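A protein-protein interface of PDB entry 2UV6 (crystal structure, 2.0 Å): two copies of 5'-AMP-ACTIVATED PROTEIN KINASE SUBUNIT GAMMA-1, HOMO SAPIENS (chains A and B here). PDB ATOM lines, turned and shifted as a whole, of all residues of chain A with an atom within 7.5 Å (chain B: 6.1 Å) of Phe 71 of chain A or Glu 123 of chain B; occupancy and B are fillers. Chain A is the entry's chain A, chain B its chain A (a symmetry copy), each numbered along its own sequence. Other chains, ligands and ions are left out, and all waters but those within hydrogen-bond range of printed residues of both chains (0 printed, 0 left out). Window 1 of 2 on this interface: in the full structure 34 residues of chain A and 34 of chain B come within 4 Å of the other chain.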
ATOM      1  N   PHE A  47     -24.197   6.626  15.660  1.00  0.00           N
ATOM      2  CA  PHE A  47     -25.476   6.282  15.056  1.00  0.00           C
ATOM      3  C   PHE A  47     -26.634   6.316  16.064  1.00  0.00           C
ATOM      4  O   PHE A  47     -27.698   6.857  15.771  1.00  0.00           O
ATOM      5  CB  PHE A  47     -25.415   4.898  14.411  1.00  0.00           C
ATOM      6  CG  PHE A  47     -24.603   4.832  13.138  1.00  0.00           C
ATOM      7  CD1 PHE A  47     -24.671   5.844  12.174  1.00  0.00           C
ATOM      8  CD2 PHE A  47     -23.793   3.727  12.882  1.00  0.00           C
ATOM      9  CE1 PHE A  47     -23.948   5.759  10.997  1.00  0.00           C
ATOM     10  CE2 PHE A  47     -23.065   3.636  11.710  1.00  0.00           C
ATOM     11  CZ  PHE A  47     -23.142   4.664  10.754  1.00  0.00           C
ATOM     12  N   SER A  53     -27.434   8.944   9.600  1.00  0.00           N
ATOM     13  CA  SER A  53     -27.630   7.652   8.904  1.00  0.00           C
ATOM     14  C   SER A  53     -26.364   7.043   8.294  1.00  0.00           C
ATOM     15  O   SER A  53     -26.314   5.845   8.001  1.00  0.00           O
ATOM     16  CB  SER A  53     -28.672   7.826   7.800  1.00  0.00           C
ATOM     17  OG  SER A  53     -28.210   8.782   6.855  1.00  0.00           O
ATOM     18  N   TYR A  68     -19.401   5.014   6.003  1.00  0.00           N
ATOM     19  CA  TYR A  68     -19.802   3.948   6.930  1.00  0.00           C
ATOM     20  C   TYR A  68     -21.252   4.166   7.320  1.00  0.00           C
ATOM     21  O   TYR A  68     -21.602   5.228   7.828  1.00  0.00           O
ATOM     22  CB  TYR A  68     -18.879   3.910   8.144  1.00  0.00           C
ATOM     23  CG  TYR A  68     -18.948   2.607   8.922  1.00  0.00           C
ATOM     24  CD1 TYR A  68     -18.217   1.497   8.527  1.00  0.00           C
ATOM     25  CD2 TYR A  68     -19.733   2.513  10.081  1.00  0.00           C
ATOM     26  CE1 TYR A  68     -18.289   0.312   9.244  1.00  0.00           C
ATOM     27  CE2 TYR A  68     -19.810   1.379  10.794  1.00  0.00           C
ATOM     28  CZ  TYR A  68     -19.083   0.258  10.388  1.00  0.00           C
ATOM     29  OH  TYR A  68     -19.186  -0.895  11.116  1.00  0.00           O
ATOM     30  N   SER A  69     -22.109   3.171   7.044  1.00  0.00           N
ATOM     31  CA  SER A  69     -23.539   3.300   7.278  1.00  0.00           C
ATOM     32  C   SER A  69     -24.014   2.320   8.343  1.00  0.00           C
ATOM     33  O   SER A  69     -23.272   1.453   8.780  1.00  0.00           O
ATOM     34  CB  SER A  69     -24.309   3.029   5.991  1.00  0.00           C
ATOM     35  OG  SER A  69     -24.169   1.675   5.602  1.00  0.00           O
ATOM     36  N   LYS A  70     -25.271   2.467   8.733  1.00  0.00           N
ATOM     37  CA  LYS A  70     -25.899   1.596   9.715  1.00  0.00           C
ATOM     38  C   LYS A  70     -25.908   0.150   9.208  1.00  0.00           C
ATOM     39  O   LYS A  70     -25.759  -0.792   9.990  1.00  0.00           O
ATOM     40  CB  LYS A  70     -27.325   2.090  10.008  1.00  0.00           C
ATOM     41  CG  LYS A  70     -27.392   3.438  10.742  1.00  0.00           C
ATOM     42  CD  LYS A  70     -28.821   3.897  10.974  1.00  0.00           C
ATOM     43  CE  LYS A  70     -28.909   5.168  11.842  1.00  0.00           C
ATOM     44  NZ  LYS A  70     -30.323   5.664  12.000  1.00  0.00           N
ATOM     45  N   PHE A  71     -26.085  -0.031   7.902  1.00  0.00           N
ATOM     46  CA  PHE A  71     -26.086  -1.381   7.316  1.00  0.00           C
ATOM     47  C   PHE A  71     -24.712  -2.061   7.472  1.00  0.00           C
ATOM     48  O   PHE A  71     -24.617  -3.254   7.708  1.00  0.00           O
ATOM     49  CB  PHE A  71     -26.562  -1.388   5.834  1.00  0.00           C
ATOM     50  CG  PHE A  71     -26.614  -2.780   5.258  1.00  0.00           C
ATOM     51  CD1 PHE A  71     -27.664  -3.625   5.570  1.00  0.00           C
ATOM     52  CD2 PHE A  71     -25.542  -3.284   4.527  1.00  0.00           C
ATOM     53  CE1 PHE A  71     -27.686  -4.955   5.096  1.00  0.00           C
ATOM     54  CE2 PHE A  71     -25.553  -4.601   4.049  1.00  0.00           C
ATOM     55  CZ  PHE A  71     -26.618  -5.435   4.343  1.00  0.00           C
ATOM     56  N   ASP A  72     -23.644  -1.284   7.393  1.00  0.00           N
ATOM     57  CA  ASP A  72     -22.304  -1.799   7.643  1.00  0.00           C
ATOM     58  C   ASP A  72     -22.135  -2.465   9.012  1.00  0.00           C
ATOM     59  O   ASP A  72     -21.438  -3.477   9.135  1.00  0.00           O
ATOM     60  CB  ASP A  72     -21.277  -0.663   7.467  1.00  0.00           C
ATOM     61  CG  ASP A  72     -21.118  -0.255   6.009  1.00  0.00           C
ATOM     62  OD1 ASP A  72     -21.278  -1.117   5.096  1.00  0.00           O
ATOM     63  OD2 ASP A  72     -20.844   0.926   5.764  1.00  0.00           O
ATOM     64  N   VAL A  73     -22.763  -1.885  10.031  1.00  0.00           N
ATOM     65  CA  VAL A  73     -22.757  -2.452  11.373  1.00  0.00           C
ATOM     66  C   VAL A  73     -23.508  -3.771  11.438  1.00  0.00           C
ATOM     67  O   VAL A  73     -23.024  -4.730  12.045  1.00  0.00           O
ATOM     68  CB  VAL A  73     -23.404  -1.479  12.386  1.00  0.00           C
ATOM     69  CG1 VAL A  73     -23.448  -2.094  13.782  1.00  0.00           C
ATOM     70  CG2 VAL A  73     -22.663  -0.175  12.375  1.00  0.00           C
ATOM     71  N   ILE A  74     -24.694  -3.809  10.824  1.00  0.00           N
ATOM     72  CA  ILE A  74     -25.505  -5.046  10.735  1.00  0.00           C
ATOM     73  C   ILE A  74     -24.769  -6.164   9.968  1.00  0.00           C
ATOM     74  O   ILE A  74     -24.779  -7.338  10.350  1.00  0.00           O
ATOM     75  CB  ILE A  74     -26.907  -4.720  10.084  1.00  0.00           C
ATOM     76  CG1 ILE A  74     -27.681  -3.705  10.942  1.00  0.00           C
ATOM     77  CG2 ILE A  74     -27.744  -5.952   9.861  1.00  0.00           C
ATOM     78  CD1 ILE A  74     -27.642  -3.964  12.405  1.00  0.00           C
ATOM     79  N   ASN A  75     -24.105  -5.783   8.896  1.00  0.00           N
ATOM     80  CA  ASN A  75     -23.293  -6.708   8.115  1.00  0.00           C
ATOM     81  C   ASN A  75     -22.128  -7.291   8.980  1.00  0.00           C
ATOM     82  O   ASN A  75     -21.902  -8.507   8.999  1.00  0.00           O
ATOM     83  CB  ASN A  75     -22.802  -5.963   6.869  1.00  0.00           C
ATOM     84  CG  ASN A  75     -22.660  -6.847   5.629  1.00  0.00           C
ATOM     85  OD1 ASN A  75     -23.036  -8.033   5.595  1.00  0.00           O
ATOM     86  ND2 ASN A  75     -22.102  -6.249   4.591  1.00  0.00           N
ATOM     87  N   LEU A  76     -21.440  -6.430   9.724  1.00  0.00           N
ATOM     88  CA  LEU A  76     -20.449  -6.831  10.728  1.00  0.00           C
ATOM     89  C   LEU A  76     -21.047  -7.803  11.741  1.00  0.00           C
ATOM     90  O   LEU A  76     -20.450  -8.840  12.062  1.00  0.00           O
ATOM     91  CB  LEU A  76     -19.871  -5.597  11.463  1.00  0.00           C
ATOM     92  CG  LEU A  76     -18.842  -5.854  12.575  1.00  0.00           C
ATOM     93  CD1 LEU A  76     -17.592  -6.517  12.003  1.00  0.00           C
ATOM     94  CD2 LEU A  76     -18.486  -4.594  13.384  1.00  0.00           C
ATOM     95  N   ALA A  77     -22.236  -7.453  12.230  1.00  0.00           N
ATOM     96  CA  ALA A  77     -22.946  -8.262  13.202  1.00  0.00           C
ATOM     97  C   ALA A  77     -23.308  -9.657  12.666  1.00  0.00           C
ATOM     98  O   ALA A  77     -23.286 -10.617  13.432  1.00  0.00           O
ATOM     99  CB  ALA A  77     -24.197  -7.499  13.722  1.00  0.00           C
ATOM    100  N   HIS A  95     -16.430  -6.007   2.295  1.00  0.00           N
ATOM    101  CA  HIS A  95     -17.735  -6.288   1.714  1.00  0.00           C
ATOM    102  C   HIS A  95     -18.043  -5.479   0.472  1.00  0.00           C
ATOM    103  O   HIS A  95     -18.854  -5.917  -0.338  1.00  0.00           O
ATOM    104  CB  HIS A  95     -18.827  -5.981   2.727  1.00  0.00           C
ATOM    105  CG  HIS A  95     -18.786  -6.850   3.935  1.00  0.00           C
ATOM    106  ND1 HIS A  95     -19.016  -8.211   3.874  1.00  0.00           N
ATOM    107  CD2 HIS A  95     -18.511  -6.565   5.227  1.00  0.00           C
ATOM    108  CE1 HIS A  95     -18.900  -8.719   5.088  1.00  0.00           C
ATOM    109  NE2 HIS A  95     -18.583  -7.744   5.924  1.00  0.00           N
ATOM    110  N   ARG A  96     -17.416  -4.308   0.332  1.00  0.00           N
ATOM    111  CA  ARG A  96     -17.685  -3.372  -0.768  1.00  0.00           C
ATOM    112  C   ARG A  96     -16.668  -2.229  -0.830  1.00  0.00           C
ATOM    113  O   ARG A  96     -16.139  -1.807   0.201  1.00  0.00           O
ATOM    114  CB  ARG A  96     -19.108  -2.782  -0.650  1.00  0.00           C
ATOM    115  CG  ARG A  96     -19.317  -1.661   0.395  1.00  0.00           C
ATOM    116  CD  ARG A  96     -19.289  -2.171   1.868  1.00  0.00           C
ATOM    117  NE  ARG A  96     -19.473  -1.055   2.798  1.00  0.00           N
ATOM    118  CZ  ARG A  96     -18.542  -0.130   3.032  1.00  0.00           C
ATOM    119  NH1 ARG A  96     -17.365  -0.178   2.411  1.00  0.00           N
ATOM    120  NH2 ARG A  96     -18.784   0.859   3.879  1.00  0.00           N
ATOM    121  N   ALA A 122     -25.148   1.444  -7.748  1.00  0.00           N
ATOM    122  CA  ALA A 122     -24.691   0.501  -6.709  1.00  0.00           C
ATOM    123  C   ALA A 122     -25.695   0.308  -5.575  1.00  0.00           C
ATOM    124  O   ALA A 122     -25.360  -0.321  -4.594  1.00  0.00           O
ATOM    125  CB  ALA A 122     -23.378   0.964  -6.130  1.00  0.00           C
ATOM    126  N   GLU A 123     -26.902   0.869  -5.705  1.00  0.00           N
ATOM    127  CA  GLU A 123     -27.914   0.802  -4.670  1.00  0.00           C
ATOM    128  C   GLU A 123     -27.376   1.333  -3.351  1.00  0.00           C
ATOM    129  O   GLU A 123     -27.430   0.653  -2.325  1.00  0.00           O
ATOM    130  CB  GLU A 123     -28.427  -0.623  -4.483  1.00  0.00           C
ATOM    131  CG  GLU A 123     -28.872  -1.276  -5.770  1.00  0.00           C
ATOM    132  CD  GLU A 123     -29.527  -2.623  -5.525  1.00  0.00           C
ATOM    133  OE1 GLU A 123     -30.756  -2.747  -5.768  1.00  0.00           O
ATOM    134  OE2 GLU A 123     -28.807  -3.539  -5.070  1.00  0.00           O
ATOM    135  N   HIS A 125     -27.416   4.723  -0.574  1.00  0.00           N
ATOM    136  CA  HIS A 125     -28.409   5.682  -0.096  1.00  0.00           C
ATOM    137  C   HIS A 125     -27.848   7.098   0.098  1.00  0.00           C
ATOM    138  O   HIS A 125     -28.589   8.008   0.454  1.00  0.00           O
ATOM    139  CB  HIS A 125     -29.030   5.184   1.207  1.00  0.00           C
ATOM    140  CG  HIS A 125     -29.897   3.967   1.046  1.00  0.00           C
ATOM    141  ND1 HIS A 125     -30.965   3.711   1.872  1.00  0.00           N
ATOM    142  CD2 HIS A 125     -29.861   2.946   0.154  1.00  0.00           C
ATOM    143  CE1 HIS A 125     -31.544   2.579   1.502  1.00  0.00           C
ATOM    144  NE2 HIS A 125     -30.888   2.091   0.467  1.00  0.00           N
ATOM    145  N   ARG B 118     -31.577 -12.189   7.877  1.00  0.00           N
ATOM    146  CA  ARG B 118     -32.564 -11.884   6.844  1.00  0.00           C
ATOM    147  C   ARG B 118     -32.321 -10.522   6.201  1.00  0.00           C
ATOM    148  O   ARG B 118     -32.321 -10.402   4.976  1.00  0.00           O
ATOM    149  CB  ARG B 118     -33.986 -11.971   7.432  1.00  0.00           C
ATOM    150  CG  ARG B 118     -35.094 -11.792   6.429  1.00  0.00           C
ATOM    151  CD  ARG B 118     -36.462 -12.105   7.040  1.00  0.00           C
ATOM    152  NE  ARG B 118     -36.488 -13.465   7.566  1.00  0.00           N
ATOM    153  CZ  ARG B 118     -37.193 -13.876   8.616  1.00  0.00           C
ATOM    154  NH1 ARG B 118     -37.984 -13.050   9.286  1.00  0.00           N
ATOM    155  NH2 ARG B 118     -37.069 -15.126   9.017  1.00  0.00           N
ATOM    156  N   LEU B 119     -32.081  -9.506   7.026  1.00  0.00           N
ATOM    157  CA  LEU B 119     -31.690  -8.175   6.538  1.00  0.00           C
ATOM    158  C   LEU B 119     -30.486  -8.233   5.605  1.00  0.00           C
ATOM    159  O   LEU B 119     -30.498  -7.640   4.513  1.00  0.00           O
ATOM    160  CB  LEU B 119     -31.367  -7.244   7.716  1.00  0.00           C
ATOM    161  CG  LEU B 119     -32.540  -6.850   8.604  1.00  0.00           C
ATOM    162  CD1 LEU B 119     -32.043  -6.160   9.882  1.00  0.00           C
ATOM    163  CD2 LEU B 119     -33.536  -5.979   7.830  1.00  0.00           C
ATOM    164  N   VAL B 120     -29.461  -8.954   6.047  1.00  0.00           N
ATOM    165  CA  VAL B 120     -28.175  -9.085   5.337  1.00  0.00           C
ATOM    166  C   VAL B 120     -28.284  -9.943   4.061  1.00  0.00           C
ATOM    167  O   VAL B 120     -27.667  -9.626   3.046  1.00  0.00           O
ATOM    168  CB  VAL B 120     -27.055  -9.609   6.316  1.00  0.00           C
ATOM    169  CG1 VAL B 120     -25.795 -10.084   5.583  1.00  0.00           C
ATOM    170  CG2 VAL B 120     -26.698  -8.524   7.310  1.00  0.00           C
ATOM    171  N   GLU B 121     -29.119 -10.979   4.116  1.00  0.00           N
ATOM    172  CA  GLU B 121     -29.458 -11.821   2.978  1.00  0.00           C
ATOM    173  C   GLU B 121     -29.802 -11.096   1.679  1.00  0.00           C
ATOM    174  O   GLU B 121     -29.343 -11.510   0.622  1.00  0.00           O
ATOM    175  CB  GLU B 121     -30.648 -12.722   3.326  1.00  0.00           C
ATOM    176  CG  GLU B 121     -30.684 -14.022   2.543  1.00  0.00           C
ATOM    177  CD  GLU B 121     -31.779 -14.973   3.010  1.00  0.00           C
ATOM    178  OE1 GLU B 121     -32.489 -14.676   4.004  1.00  0.00           O
ATOM    179  OE2 GLU B 121     -31.923 -16.032   2.367  1.00  0.00           O
ATOM    180  N   ALA B 122     -30.643 -10.064   1.753  1.00  0.00           N
ATOM    181  CA  ALA B 122     -31.028  -9.280   0.562  1.00  0.00           C
ATOM    182  C   ALA B 122     -30.605  -7.815   0.633  1.00  0.00           C
ATOM    183  O   ALA B 122     -31.003  -7.047  -0.216  1.00  0.00           O
ATOM    184  CB  ALA B 122     -32.518  -9.353   0.353  1.00  0.00           C
ATOM    185  N   GLU B 123     -29.828  -7.436   1.653  1.00  0.00           N
ATOM    186  CA  GLU B 123     -29.413  -6.062   1.855  1.00  0.00           C
ATOM    187  C   GLU B 123     -30.617  -5.136   1.916  1.00  0.00           C
ATOM    188  O   GLU B 123     -30.700  -4.155   1.175  1.00  0.00           O
ATOM    189  CB  GLU B 123     -28.459  -5.600   0.757  1.00  0.00           C
ATOM    190  CG  GLU B 123     -27.290  -6.531   0.543  1.00  0.00           C
ATOM    191  CD  GLU B 123     -26.281  -5.960  -0.435  1.00  0.00           C
ATOM    192  OE1 GLU B 123     -25.143  -5.638  -0.005  1.00  0.00           O
ATOM    193  OE2 GLU B 123     -26.648  -5.817  -1.622  1.00  0.00           O
ATOM    194  N   VAL B 124     -31.548  -5.474   2.803  1.00  0.00           N
ATOM    195  CA  VAL B 124     -32.719  -4.637   3.060  1.00  0.00           C
ATOM    196  C   VAL B 124     -32.576  -3.964   4.428  1.00  0.00           C
ATOM    197  O   VAL B 124     -31.890  -4.484   5.327  1.00  0.00           O
ATOM    198  CB  VAL B 124     -34.046  -5.458   2.953  1.00  0.00           C
ATOM    199  CG1 VAL B 124     -34.227  -5.972   1.522  1.00  0.00           C
ATOM    200  CG2 VAL B 124     -34.086  -6.599   3.974  1.00  0.00           C
ATOM    201  N   HIS B 125     -33.198  -2.790   4.570  1.00  0.00           N
ATOM    202  CA  HIS B 125     -33.015  -1.978   5.770  1.00  0.00           C
ATOM    203  C   HIS B 125     -34.160  -2.118   6.784  1.00  0.00           C
ATOM    204  O   HIS B 125     -34.107  -1.522   7.855  1.00  0.00           O
ATOM    205  CB  HIS B 125     -32.837  -0.511   5.384  1.00  0.00           C
ATOM    206  CG  HIS B 125     -31.548  -0.219   4.670  1.00  0.00           C
ATOM    207  ND1 HIS B 125     -30.920   1.000   4.756  1.00  0.00           N
ATOM    208  CD2 HIS B 125     -30.766  -0.986   3.869  1.00  0.00           C
ATOM    209  CE1 HIS B 125     -29.812   0.976   4.031  1.00  0.00           C
ATOM    210  NE2 HIS B 125     -29.700  -0.216   3.475  1.00  0.00           N
ATOM    211  N   LEU B 142     -33.093  -0.744  10.716  1.00  0.00           N
ATOM    212  CA  LEU B 142     -31.709  -0.853  11.207  1.00  0.00           C
ATOM    213  C   LEU B 142     -31.480  -0.017  12.486  1.00  0.00           C
ATOM    214  O   LEU B 142     -30.773  -0.462  13.373  1.00  0.00           O
ATOM    215  CB  LEU B 142     -30.696  -0.429  10.142  1.00  0.00           C
ATOM    216  CG  LEU B 142     -30.772  -1.078   8.757  1.00  0.00           C
ATOM    217  CD1 LEU B 142     -29.664  -0.525   7.881  1.00  0.00           C
ATOM    218  CD2 LEU B 142     -30.690  -2.602   8.868  1.00  0.00           C
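The backbone carbonyl oxygen (O) of Leu 119 of chain B lies within hydrogen-bond range of the backbone NH (N) of Val 124 of chain B (3.0 Å). OG of Ser 69 of chain A sits close to N of Phe 71 of chain A (3.4 Å). N of Leu 142 of chain B is in hydrogen-bond range of O of His 125 of chain B (3.1 Å).
Among the printed residues, merely in contact across the chains: Asn 75 of chain A with Val 120 of chain B, His 125 of chain A with His 125 of chain B, Phe 71 of chain A with Leu 142 of chain B, Ile 74 of chain A with Val 120 of chain B, Phe 71 of chain A with Glu 123 of chain B, Ile 74 of chain A with Leu 142 of chain B and Phe 71 of chain A with Leu 119 of chain B.
Of the printed residues of chain B, Asn 75 of chain A touches Val 120. Printed residues of chain B within 4 Å of His 125 of chain A: His 125. Of the printed residues of chain A, Leu 119 of chain B touches Phe 71. Printed residues of chain A within 4 Å of Val 120 of chain B: Ile 74 and Asn 75. Glu 123 of chain B touches one residue of chain A. Printed residues of chain A within 4 Å of His 125 of chain B: His 125 (3.5 Å). The nearest printed residue of chain B that does not touch Phe 71 of chain A is Val 120 of chain B (4.1 Å). The nearest printed residue of chain A that does not touch Val 120 of chain B is Phe 71 of chain A (4.1 Å).
Of the 9 printed residues of chain B, 5 touch a printed residue of chain A. Among the printed residues, no Asp or Glu carboxylate lies within 4 Å of a Lys or Arg side-chain nitrogen of the other chain.
His 125 of chain A touches its own counterpart, His 125 of chain B. Of the 7 pairs that touch across the chains among the printed residues, 1 has its exchanged pair printed and touching as well.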
